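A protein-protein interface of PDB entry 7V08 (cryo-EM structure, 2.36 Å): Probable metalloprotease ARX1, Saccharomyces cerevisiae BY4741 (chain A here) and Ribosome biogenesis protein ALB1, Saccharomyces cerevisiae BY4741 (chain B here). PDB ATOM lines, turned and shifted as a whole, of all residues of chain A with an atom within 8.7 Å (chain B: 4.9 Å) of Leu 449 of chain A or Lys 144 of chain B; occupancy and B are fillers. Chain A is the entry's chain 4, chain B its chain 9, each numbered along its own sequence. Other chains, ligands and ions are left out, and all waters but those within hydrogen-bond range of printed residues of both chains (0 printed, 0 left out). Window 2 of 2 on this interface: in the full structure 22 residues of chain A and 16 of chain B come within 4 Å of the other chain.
Lys 144 of chain B touches just one residue of chain A: Leu 449 (2.4 Å). Of the printed residues of chain A, Trp 148 of chain B touches Leu 449. Of the printed residues of chain A, Leu 147 of chain B touches Leu 278 (3.7 Å) and Leu 478 (3.8 Å). Lys 450 of chain A touches none of the printed residues of chain B. The nearest residue of chain B that does not touch Leu 449 of chain A is Ile 151 of chain B (4.02 Å). The nearest residue of chain A that does not touch Lys 144 of chain B is Leu 478 of chain A (4.1 Å).
Among the printed residues, merely in contact across the chains: Leu 449 of chain A with Trp 148 of chain B (3.5 Å), Leu 278 of chain A with Leu 147 of chain B (3.7 Å), Leu 478 of chain A with Val 143 of chain B (3.7 Å) and Leu 478 of chain A with Leu 147 of chain B (3.8 Å).
Of the 21 printed residues of chain A, 3 touch a printed residue of chain B. Hydrophobic or aromatic side chains of chain A within 4 Å of the printed part of chain B: Leu 278, Leu 449 and Leu 478. Hydrophobic or aromatic side chains of chain B that line the printed part of chain A: Val 143, Leu 147 and Trp 148.
The backbone carbonyl oxygen (O) of Leu 449 of chain A lies within hydrogen-bond range of the side-chain amino group (NZ) of Lys 144 of chain B.
The backbone NH (N) of Leu 478 of chain A sits close to the side-chain carboxylate (OE2) of Glu 275 of chain A, at 3.4 Å.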
ATOM      1  N   GLU A 275     -18.982  20.170 -17.373  1.00  0.00           N
ATOM      2  CA  GLU A 275     -20.092  19.946 -16.453  1.00  0.00           C
ATOM      3  C   GLU A 275     -19.778  20.496 -15.068  1.00  0.00           C
ATOM      4  O   GLU A 275     -20.617  21.163 -14.449  1.00  0.00           O
ATOM      5  CB  GLU A 275     -20.405  18.455 -16.381  1.00  0.00           C
ATOM      6  CG  GLU A 275     -21.595  18.087 -15.523  1.00  0.00           C
ATOM      7  CD  GLU A 275     -21.711  16.589 -15.322  1.00  0.00           C
ATOM      8  OE1 GLU A 275     -20.749  15.980 -14.804  1.00  0.00           O
ATOM      9  OE2 GLU A 275     -22.755  16.020 -15.700  1.00  0.00           O
ATOM     10  N   LEU A 278     -19.849  24.387 -15.158  1.00  0.00           N
ATOM     11  CA  LEU A 278     -21.217  24.901 -15.164  1.00  0.00           C
ATOM     12  C   LEU A 278     -21.885  24.703 -13.809  1.00  0.00           C
ATOM     13  O   LEU A 278     -22.679  25.543 -13.369  1.00  0.00           O
ATOM     14  CB  LEU A 278     -22.035  24.224 -16.263  1.00  0.00           C
ATOM     15  CG  LEU A 278     -23.397  24.850 -16.575  1.00  0.00           C
ATOM     16  CD1 LEU A 278     -23.227  26.264 -17.113  1.00  0.00           C
ATOM     17  CD2 LEU A 278     -24.167  23.990 -17.561  1.00  0.00           C
ATOM     18  N   LEU A 279     -21.583  23.592 -13.136  1.00  0.00           N
ATOM     19  CA  LEU A 279     -22.152  23.333 -11.823  1.00  0.00           C
ATOM     20  C   LEU A 279     -21.584  24.244 -10.744  1.00  0.00           C
ATOM     21  O   LEU A 279     -22.281  24.534  -9.766  1.00  0.00           O
ATOM     22  CB  LEU A 279     -21.915  21.870 -11.446  1.00  0.00           C
ATOM     23  CG  LEU A 279     -22.604  21.329 -10.202  1.00  0.00           C
ATOM     24  CD1 LEU A 279     -24.041  20.970 -10.514  1.00  0.00           C
ATOM     25  CD2 LEU A 279     -21.844  20.128  -9.663  1.00  0.00           C
ATOM     26  N   LYS A 332     -26.885  27.918 -23.846  1.00  0.00           N
ATOM     27  CA  LYS A 332     -25.746  27.305 -23.178  1.00  0.00           C
ATOM     28  C   LYS A 332     -25.709  25.828 -23.541  1.00  0.00           C
ATOM     29  O   LYS A 332     -26.693  25.109 -23.342  1.00  0.00           O
ATOM     30  CB  LYS A 332     -25.825  27.491 -21.665  1.00  0.00           C
ATOM     31  CG  LYS A 332     -24.670  28.294 -21.103  1.00  0.00           C
ATOM     32  CD  LYS A 332     -24.806  28.505 -19.606  1.00  0.00           C
ATOM     33  CE  LYS A 332     -25.801  29.604 -19.284  1.00  0.00           C
ATOM     34  NZ  LYS A 332     -25.623  30.111 -17.894  1.00  0.00           N
ATOM     35  N   VAL A 443     -23.777  20.626 -28.342  1.00  0.00           N
ATOM     36  CA  VAL A 443     -25.050  20.044 -27.936  1.00  0.00           C
ATOM     37  C   VAL A 443     -25.632  20.905 -26.822  1.00  0.00           C
ATOM     38  O   VAL A 443     -24.983  21.094 -25.790  1.00  0.00           O
ATOM     39  CB  VAL A 443     -24.912  18.585 -27.468  1.00  0.00           C
ATOM     40  CG1 VAL A 443     -26.277  18.027 -27.075  1.00  0.00           C
ATOM     41  CG2 VAL A 443     -24.283  17.735 -28.547  1.00  0.00           C
ATOM     42  N   PRO A 444     -26.839  21.445 -26.979  1.00  0.00           N
ATOM     43  CA  PRO A 444     -27.428  22.262 -25.912  1.00  0.00           C
ATOM     44  C   PRO A 444     -27.780  21.437 -24.684  1.00  0.00           C
ATOM     45  O   PRO A 444     -28.074  20.243 -24.772  1.00  0.00           O
ATOM     46  CB  PRO A 444     -28.683  22.846 -26.568  1.00  0.00           C
ATOM     47  CG  PRO A 444     -29.020  21.898 -27.652  1.00  0.00           C
ATOM     48  CD  PRO A 444     -27.715  21.351 -28.157  1.00  0.00           C
ATOM     49  N   TRP A 445     -27.752  22.100 -23.525  1.00  0.00           N
ATOM     50  CA  TRP A 445     -27.927  21.404 -22.253  1.00  0.00           C
ATOM     51  C   TRP A 445     -29.370  20.977 -22.011  1.00  0.00           C
ATOM     52  O   TRP A 445     -29.606  19.998 -21.292  1.00  0.00           O
ATOM     53  CB  TRP A 445     -27.458  22.281 -21.091  1.00  0.00           C
ATOM     54  CG  TRP A 445     -25.978  22.363 -20.925  1.00  0.00           C
ATOM     55  CD1 TRP A 445     -25.176  23.403 -21.277  1.00  0.00           C
ATOM     56  CD2 TRP A 445     -25.122  21.375 -20.347  1.00  0.00           C
ATOM     57  NE1 TRP A 445     -23.870  23.122 -20.968  1.00  0.00           N
ATOM     58  CE2 TRP A 445     -23.810  21.883 -20.390  1.00  0.00           C
ATOM     59  CE3 TRP A 445     -25.337  20.108 -19.795  1.00  0.00           C
ATOM     60  CZ2 TRP A 445     -22.716  21.168 -19.912  1.00  0.00           C
ATOM     61  CZ3 TRP A 445     -24.252  19.403 -19.318  1.00  0.00           C
ATOM     62  CH2 TRP A 445     -22.957  19.935 -19.378  1.00  0.00           C
ATOM     63  N   ASP A 446     -30.344  21.706 -22.564  1.00  0.00           N
ATOM     64  CA  ASP A 446     -31.743  21.367 -22.315  1.00  0.00           C
ATOM     65  C   ASP A 446     -32.111  20.024 -22.935  1.00  0.00           C
ATOM     66  O   ASP A 446     -32.886  19.259 -22.351  1.00  0.00           O
ATOM     67  CB  ASP A 446     -32.659  22.479 -22.824  1.00  0.00           C
ATOM     68  CG  ASP A 446     -32.312  22.939 -24.226  1.00  0.00           C
ATOM     69  OD1 ASP A 446     -31.473  22.296 -24.885  1.00  0.00           O
ATOM     70  OD2 ASP A 446     -32.880  23.959 -24.664  1.00  0.00           O
ATOM     71  N   HIS A 447     -31.552  19.712 -24.106  1.00  0.00           N
ATOM     72  CA  HIS A 447     -31.777  18.406 -24.715  1.00  0.00           C
ATOM     73  C   HIS A 447     -31.207  17.285 -23.851  1.00  0.00           C
ATOM     74  O   HIS A 447     -31.853  16.246 -23.663  1.00  0.00           O
ATOM     75  CB  HIS A 447     -31.165  18.390 -26.113  1.00  0.00           C
ATOM     76  CG  HIS A 447     -31.354  17.104 -26.851  1.00  0.00           C
ATOM     77  ND1 HIS A 447     -32.581  16.489 -26.973  1.00  0.00           N
ATOM     78  CD2 HIS A 447     -30.474  16.326 -27.524  1.00  0.00           C
ATOM     79  CE1 HIS A 447     -32.446  15.380 -27.678  1.00  0.00           C
ATOM     80  NE2 HIS A 447     -31.179  15.261 -28.029  1.00  0.00           N
ATOM     81  N   ILE A 448     -30.007  17.488 -23.300  1.00  0.00           N
ATOM     82  CA  ILE A 448     -29.387  16.488 -22.430  1.00  0.00           C
ATOM     83  C   ILE A 448     -30.214  16.291 -21.168  1.00  0.00           C
ATOM     84  O   ILE A 448     -30.415  15.161 -20.708  1.00  0.00           O
ATOM     85  CB  ILE A 448     -27.942  16.899 -22.095  1.00  0.00           C
ATOM     86  CG1 ILE A 448     -27.125  17.077 -23.371  1.00  0.00           C
ATOM     87  CG2 ILE A 448     -27.282  15.877 -21.173  1.00  0.00           C
ATOM     88  CD1 ILE A 448     -25.787  17.705 -23.144  1.00  0.00           C
ATOM     89  N   LEU A 449     -30.696  17.389 -20.583  1.00  0.00           N
ATOM     90  CA  LEU A 449     -31.497  17.299 -19.368  1.00  0.00           C
ATOM     91  C   LEU A 449     -32.842  16.627 -19.616  1.00  0.00           C
ATOM     92  O   LEU A 449     -33.287  15.818 -18.796  1.00  0.00           O
ATOM     93  CB  LEU A 449     -31.692  18.693 -18.776  1.00  0.00           C
ATOM     94  CG  LEU A 449     -30.439  19.281 -18.127  1.00  0.00           C
ATOM     95  CD1 LEU A 449     -30.506  20.797 -18.046  1.00  0.00           C
ATOM     96  CD2 LEU A 449     -30.247  18.683 -16.748  1.00  0.00           C
ATOM     97  N   LYS A 450     -33.503  16.938 -20.728  1.00  0.00           N
ATOM     98  CA  LYS A 450     -34.790  16.320 -21.016  1.00  0.00           C
ATOM     99  C   LYS A 450     -34.670  14.878 -21.482  1.00  0.00           C
ATOM    100  O   LYS A 450     -35.643  14.128 -21.363  1.00  0.00           O
ATOM    101  CB  LYS A 450     -35.541  17.128 -22.069  1.00  0.00           C
ATOM    102  CG  LYS A 450     -36.051  18.467 -21.575  1.00  0.00           C
ATOM    103  CD  LYS A 450     -36.646  19.267 -22.729  1.00  0.00           C
ATOM    104  CE  LYS A 450     -37.350  20.519 -22.232  1.00  0.00           C
ATOM    105  NZ  LYS A 450     -37.760  21.399 -23.356  1.00  0.00           N
ATOM    106  N   ALA A 451     -33.519  14.475 -22.008  1.00  0.00           N
ATOM    107  CA  ALA A 451     -33.370  13.117 -22.500  1.00  0.00           C
ATOM    108  C   ALA A 451     -33.312  12.117 -21.348  1.00  0.00           C
ATOM    109  O   ALA A 451     -32.790  12.399 -20.266  1.00  0.00           O
ATOM    110  CB  ALA A 451     -32.114  12.997 -23.356  1.00  0.00           C
ATOM    111  N   THR A 452     -33.843  10.925 -21.603  1.00  0.00           N
ATOM    112  CA  THR A 452     -33.904   9.857 -20.617  1.00  0.00           C
ATOM    113  C   THR A 452     -33.057   8.678 -21.070  1.00  0.00           C
ATOM    114  O   THR A 452     -33.214   8.185 -22.192  1.00  0.00           O
ATOM    115  CB  THR A 452     -35.349   9.397 -20.386  1.00  0.00           C
ATOM    116  OG1 THR A 452     -35.961   9.083 -21.645  1.00  0.00           O
ATOM    117  CG2 THR A 452     -36.145  10.487 -19.712  1.00  0.00           C
ATOM    118  N   ASN A 453     -32.165   8.227 -20.196  1.00  0.00           N
ATOM    119  CA  ASN A 453     -31.319   7.064 -20.461  1.00  0.00           C
ATOM    120  C   ASN A 453     -31.626   5.974 -19.446  1.00  0.00           C
ATOM    121  O   ASN A 453     -31.268   6.116 -18.258  1.00  0.00           O
ATOM    122  CB  ASN A 453     -29.837   7.434 -20.436  1.00  0.00           C
ATOM    123  CG  ASN A 453     -29.465   8.294 -19.255  1.00  0.00           C
ATOM    124  OD1 ASN A 453     -30.296   9.018 -18.712  1.00  0.00           O
ATOM    125  ND2 ASN A 453     -28.207   8.218 -18.845  1.00  0.00           N
ATOM    126  N   LEU A 475     -19.900  12.522 -18.629  1.00  0.00           N
ATOM    127  CA  LEU A 475     -20.695  13.207 -17.610  1.00  0.00           C
ATOM    128  C   LEU A 475     -20.824  12.300 -16.394  1.00  0.00           C
ATOM    129  O   LEU A 475     -21.820  11.581 -16.242  1.00  0.00           O
ATOM    130  CB  LEU A 475     -22.062  13.614 -18.164  1.00  0.00           C
ATOM    131  CG  LEU A 475     -22.019  14.531 -19.390  1.00  0.00           C
ATOM    132  CD1 LEU A 475     -23.410  14.782 -19.942  1.00  0.00           C
ATOM    133  CD2 LEU A 475     -21.335  15.840 -19.050  1.00  0.00           C
ATOM    134  N   LYS A 477     -21.393  13.112 -13.289  1.00  0.00           N
ATOM    135  CA  LYS A 477     -22.453  13.526 -12.377  1.00  0.00           C
ATOM    136  C   LYS A 477     -23.837  13.160 -12.892  1.00  0.00           C
ATOM    137  O   LYS A 477     -24.728  12.855 -12.093  1.00  0.00           O
ATOM    138  CB  LYS A 477     -22.377  15.032 -12.121  1.00  0.00           C
ATOM    139  CG  LYS A 477     -21.103  15.471 -11.427  1.00  0.00           C
ATOM    140  CD  LYS A 477     -20.964  16.981 -11.434  1.00  0.00           C
ATOM    141  CE  LYS A 477     -19.544  17.401 -11.096  1.00  0.00           C
ATOM    142  NZ  LYS A 477     -18.564  16.678 -11.954  1.00  0.00           N
ATOM    143  N   LEU A 478     -24.045  13.192 -14.204  1.00  0.00           N
ATOM    144  CA  LEU A 478     -25.352  12.902 -14.772  1.00  0.00           C
ATOM    145  C   LEU A 478     -25.523  11.452 -15.199  1.00  0.00           C
ATOM    146  O   LEU A 478     -26.631  11.067 -15.584  1.00  0.00           O
ATOM    147  CB  LEU A 478     -25.616  13.815 -15.968  1.00  0.00           C
ATOM    148  CG  LEU A 478     -25.901  15.267 -15.605  1.00  0.00           C
ATOM    149  CD1 LEU A 478     -25.960  16.113 -16.861  1.00  0.00           C
ATOM    150  CD2 LEU A 478     -27.195  15.362 -14.823  1.00  0.00           C
ATOM    151  N   GLY A 479     -24.469  10.646 -15.141  1.00  0.00           N
ATOM    152  CA  GLY A 479     -24.563   9.269 -15.598  1.00  0.00           C
ATOM    153  C   GLY A 479     -24.837   9.126 -17.080  1.00  0.00           C
ATOM    154  O   GLY A 479     -25.562   8.212 -17.489  1.00  0.00           O
ATOM    155  N   VAL A 480     -24.270  10.011 -17.897  1.00  0.00           N
ATOM    156  CA  VAL A 480     -24.423   9.963 -19.347  1.00  0.00           C
ATOM    157  C   VAL A 480     -23.112   9.469 -19.940  1.00  0.00           C
ATOM    158  O   VAL A 480     -22.059  10.084 -19.737  1.00  0.00           O
ATOM    159  CB  VAL A 480     -24.810  11.330 -19.933  1.00  0.00           C
ATOM    160  CG1 VAL A 480     -24.801  11.274 -21.449  1.00  0.00           C
ATOM    161  CG2 VAL A 480     -26.177  11.765 -19.430  1.00  0.00           C
ATOM    162  N   LEU A 488     -27.567  11.454 -28.342  1.00  0.00           N
ATOM    163  CA  LEU A 488     -28.224  12.746 -28.137  1.00  0.00           C
ATOM    164  C   LEU A 488     -27.766  13.778 -29.160  1.00  0.00           C
ATOM    165  O   LEU A 488     -28.583  14.549 -29.688  1.00  0.00           O
ATOM    166  CB  LEU A 488     -27.956  13.268 -26.725  1.00  0.00           C
ATOM    167  CG  LEU A 488     -28.352  12.358 -25.572  1.00  0.00           C
ATOM    168  CD1 LEU A 488     -28.163  13.050 -24.239  1.00  0.00           C
ATOM    169  CD2 LEU A 488     -29.775  11.885 -25.763  1.00  0.00           C
ATOM    170  N   SER B 139     -29.782  12.548  -5.505  1.00  0.00           N
ATOM    171  CA  SER B 139     -28.657  13.329  -6.007  1.00  0.00           C
ATOM    172  C   SER B 139     -28.828  13.667  -7.482  1.00  0.00           C
ATOM    173  O   SER B 139     -28.482  14.773  -7.910  1.00  0.00           O
ATOM    174  CB  SER B 139     -27.347  12.583  -5.768  1.00  0.00           C
ATOM    175  OG  SER B 139     -26.234  13.438  -5.966  1.00  0.00           O
ATOM    176  N   LEU B 140     -29.359  12.733  -8.274  1.00  0.00           N
ATOM    177  CA  LEU B 140     -29.625  13.023  -9.679  1.00  0.00           C
ATOM    178  C   LEU B 140     -30.664  14.128  -9.822  1.00  0.00           C
ATOM    179  O   LEU B 140     -30.507  15.034 -10.651  1.00  0.00           O
ATOM    180  CB  LEU B 140     -30.085  11.756 -10.396  1.00  0.00           C
ATOM    181  CG  LEU B 140     -30.539  11.913 -11.850  1.00  0.00           C
ATOM    182  CD1 LEU B 140     -29.424  12.491 -12.706  1.00  0.00           C
ATOM    183  CD2 LEU B 140     -31.003  10.576 -12.407  1.00  0.00           C
ATOM    184  N   THR B 141     -31.723  14.075  -9.007  1.00  0.00           N
ATOM    185  CA  THR B 141     -32.745  15.117  -9.027  1.00  0.00           C
ATOM    186  C   THR B 141     -32.155  16.473  -8.664  1.00  0.00           C
ATOM    187  O   THR B 141     -32.431  17.480  -9.331  1.00  0.00           O
ATOM    188  CB  THR B 141     -33.877  14.744  -8.062  1.00  0.00           C
ATOM    189  OG1 THR B 141     -34.684  13.708  -8.635  1.00  0.00           O
ATOM    190  CG2 THR B 141     -34.750  15.945  -7.737  1.00  0.00           C
ATOM    191  N   LEU B 142     -31.322  16.514  -7.623  1.00  0.00           N
ATOM    192  CA  LEU B 142     -30.740  17.780  -7.188  1.00  0.00           C
ATOM    193  C   LEU B 142     -29.764  18.332  -8.219  1.00  0.00           C
ATOM    194  O   LEU B 142     -29.737  19.541  -8.468  1.00  0.00           O
ATOM    195  CB  LEU B 142     -30.065  17.607  -5.830  1.00  0.00           C
ATOM    196  CG  LEU B 142     -31.073  17.424  -4.695  1.00  0.00           C
ATOM    197  CD1 LEU B 142     -30.372  17.303  -3.348  1.00  0.00           C
ATOM    198  CD2 LEU B 142     -32.066  18.577  -4.694  1.00  0.00           C
ATOM    199  N   VAL B 143     -28.958  17.464  -8.833  1.00  0.00           N
ATOM    200  CA  VAL B 143     -28.025  17.909  -9.866  1.00  0.00           C
ATOM    201  C   VAL B 143     -28.782  18.442 -11.077  1.00  0.00           C
ATOM    202  O   VAL B 143     -28.420  19.480 -11.647  1.00  0.00           O
ATOM    203  CB  VAL B 143     -27.066  16.761 -10.239  1.00  0.00           C
ATOM    204  CG1 VAL B 143     -26.378  17.026 -11.564  1.00  0.00           C
ATOM    205  CG2 VAL B 143     -26.034  16.573  -9.140  1.00  0.00           C
ATOM    206  N   LYS B 144     -29.856  17.753 -11.476  1.00  0.00           N
ATOM    207  CA  LYS B 144     -30.649  18.215 -12.609  1.00  0.00           C
ATOM    208  C   LYS B 144     -31.307  19.556 -12.318  1.00  0.00           C
ATOM    209  O   LYS B 144     -31.316  20.445 -13.177  1.00  0.00           O
ATOM    210  CB  LYS B 144     -31.699  17.171 -12.976  1.00  0.00           C
ATOM    211  CG  LYS B 144     -31.146  15.968 -13.714  1.00  0.00           C
ATOM    212  CD  LYS B 144     -32.259  15.009 -14.070  1.00  0.00           C
ATOM    213  CE  LYS B 144     -33.169  15.592 -15.138  1.00  0.00           C
ATOM    214  NZ  LYS B 144     -32.543  15.516 -16.485  1.00  0.00           N
ATOM    215  N   GLU B 145     -31.850  19.732 -11.110  1.00  0.00           N
ATOM    216  CA  GLU B 145     -32.475  21.007 -10.777  1.00  0.00           C
ATOM    217  C   GLU B 145     -31.440  22.123 -10.660  1.00  0.00           C
ATOM    218  O   GLU B 145     -31.719  23.273 -11.015  1.00  0.00           O
ATOM    219  CB  GLU B 145     -33.296  20.881  -9.493  1.00  0.00           C
ATOM    220  CG  GLU B 145     -34.712  20.360  -9.713  1.00  0.00           C
ATOM    221  CD  GLU B 145     -35.586  21.325 -10.509  1.00  0.00           C
ATOM    222  OE1 GLU B 145     -35.286  22.540 -10.522  1.00  0.00           O
ATOM    223  OE2 GLU B 145     -36.576  20.866 -11.123  1.00  0.00           O
ATOM    224  N   ALA B 146     -30.239  21.805 -10.166  1.00  0.00           N
ATOM    225  CA  ALA B 146     -29.175  22.802 -10.109  1.00  0.00           C
ATOM    226  C   ALA B 146     -28.754  23.245 -11.503  1.00  0.00           C
ATOM    227  O   ALA B 146     -28.556  24.442 -11.750  1.00  0.00           O
ATOM    228  CB  ALA B 146     -27.977  22.247  -9.342  1.00  0.00           C
ATOM    229  N   LEU B 147     -28.615  22.292 -12.430  1.00  0.00           N
ATOM    230  CA  LEU B 147     -28.289  22.645 -13.808  1.00  0.00           C
ATOM    231  C   LEU B 147     -29.406  23.460 -14.447  1.00  0.00           C
ATOM    232  O   LEU B 147     -29.139  24.411 -15.191  1.00  0.00           O
ATOM    233  CB  LEU B 147     -28.014  21.385 -14.627  1.00  0.00           C
ATOM    234  CG  LEU B 147     -26.608  20.800 -14.525  1.00  0.00           C
ATOM    235  CD1 LEU B 147     -26.449  19.609 -15.452  1.00  0.00           C
ATOM    236  CD2 LEU B 147     -25.585  21.870 -14.838  1.00  0.00           C
ATOM    237  N   TRP B 148     -30.662  23.095 -14.176  1.00  0.00           N
ATOM    238  CA  TRP B 148     -31.791  23.839 -14.720  1.00  0.00           C
ATOM    239  C   TRP B 148     -31.805  25.272 -14.204  1.00  0.00           C
ATOM    240  O   TRP B 148     -32.028  26.216 -14.969  1.00  0.00           O
ATOM    241  CB  TRP B 148     -33.092  23.123 -14.369  1.00  0.00           C
ATOM    242  CG  TRP B 148     -34.220  23.442 -15.282  1.00  0.00           C
ATOM    243  CD1 TRP B 148     -35.243  24.313 -15.047  1.00  0.00           C
ATOM    244  CD2 TRP B 148     -34.446  22.900 -16.588  1.00  0.00           C
ATOM    245  NE1 TRP B 148     -36.096  24.342 -16.125  1.00  0.00           N
ATOM    246  CE2 TRP B 148     -35.628  23.482 -17.084  1.00  0.00           C
ATOM    247  CE3 TRP B 148     -33.765  21.973 -17.384  1.00  0.00           C
ATOM    248  CZ2 TRP B 148     -36.143  23.171 -18.339  1.00  0.00           C
ATOM    249  CZ3 TRP B 148     -34.280  21.666 -18.632  1.00  0.00           C
ATOM    250  CH2 TRP B 148     -35.453  22.264 -19.097  1.00  0.00           C
ATOM    251  N   ILE B 151     -28.768  27.211 -15.956  1.00  0.00           N
ATOM    252  CA  ILE B 151     -28.987  27.592 -17.348  1.00  0.00           C
ATOM    253  C   ILE B 151     -30.229  28.457 -17.523  1.00  0.00           C
ATOM    254  O   ILE B 151     -30.384  29.094 -18.572  1.00  0.00           O
ATOM    255  CB  ILE B 151     -29.071  26.364 -18.274  1.00  0.00           C
ATOM    256  CG1 ILE B 151     -30.418  25.651 -18.136  1.00  0.00           C
ATOM    257  CG2 ILE B 151     -27.913  25.412 -18.002  1.00  0.00           C
ATOM    258  CD1 ILE B 151     -30.680  24.635 -19.231  1.00  0.00           C
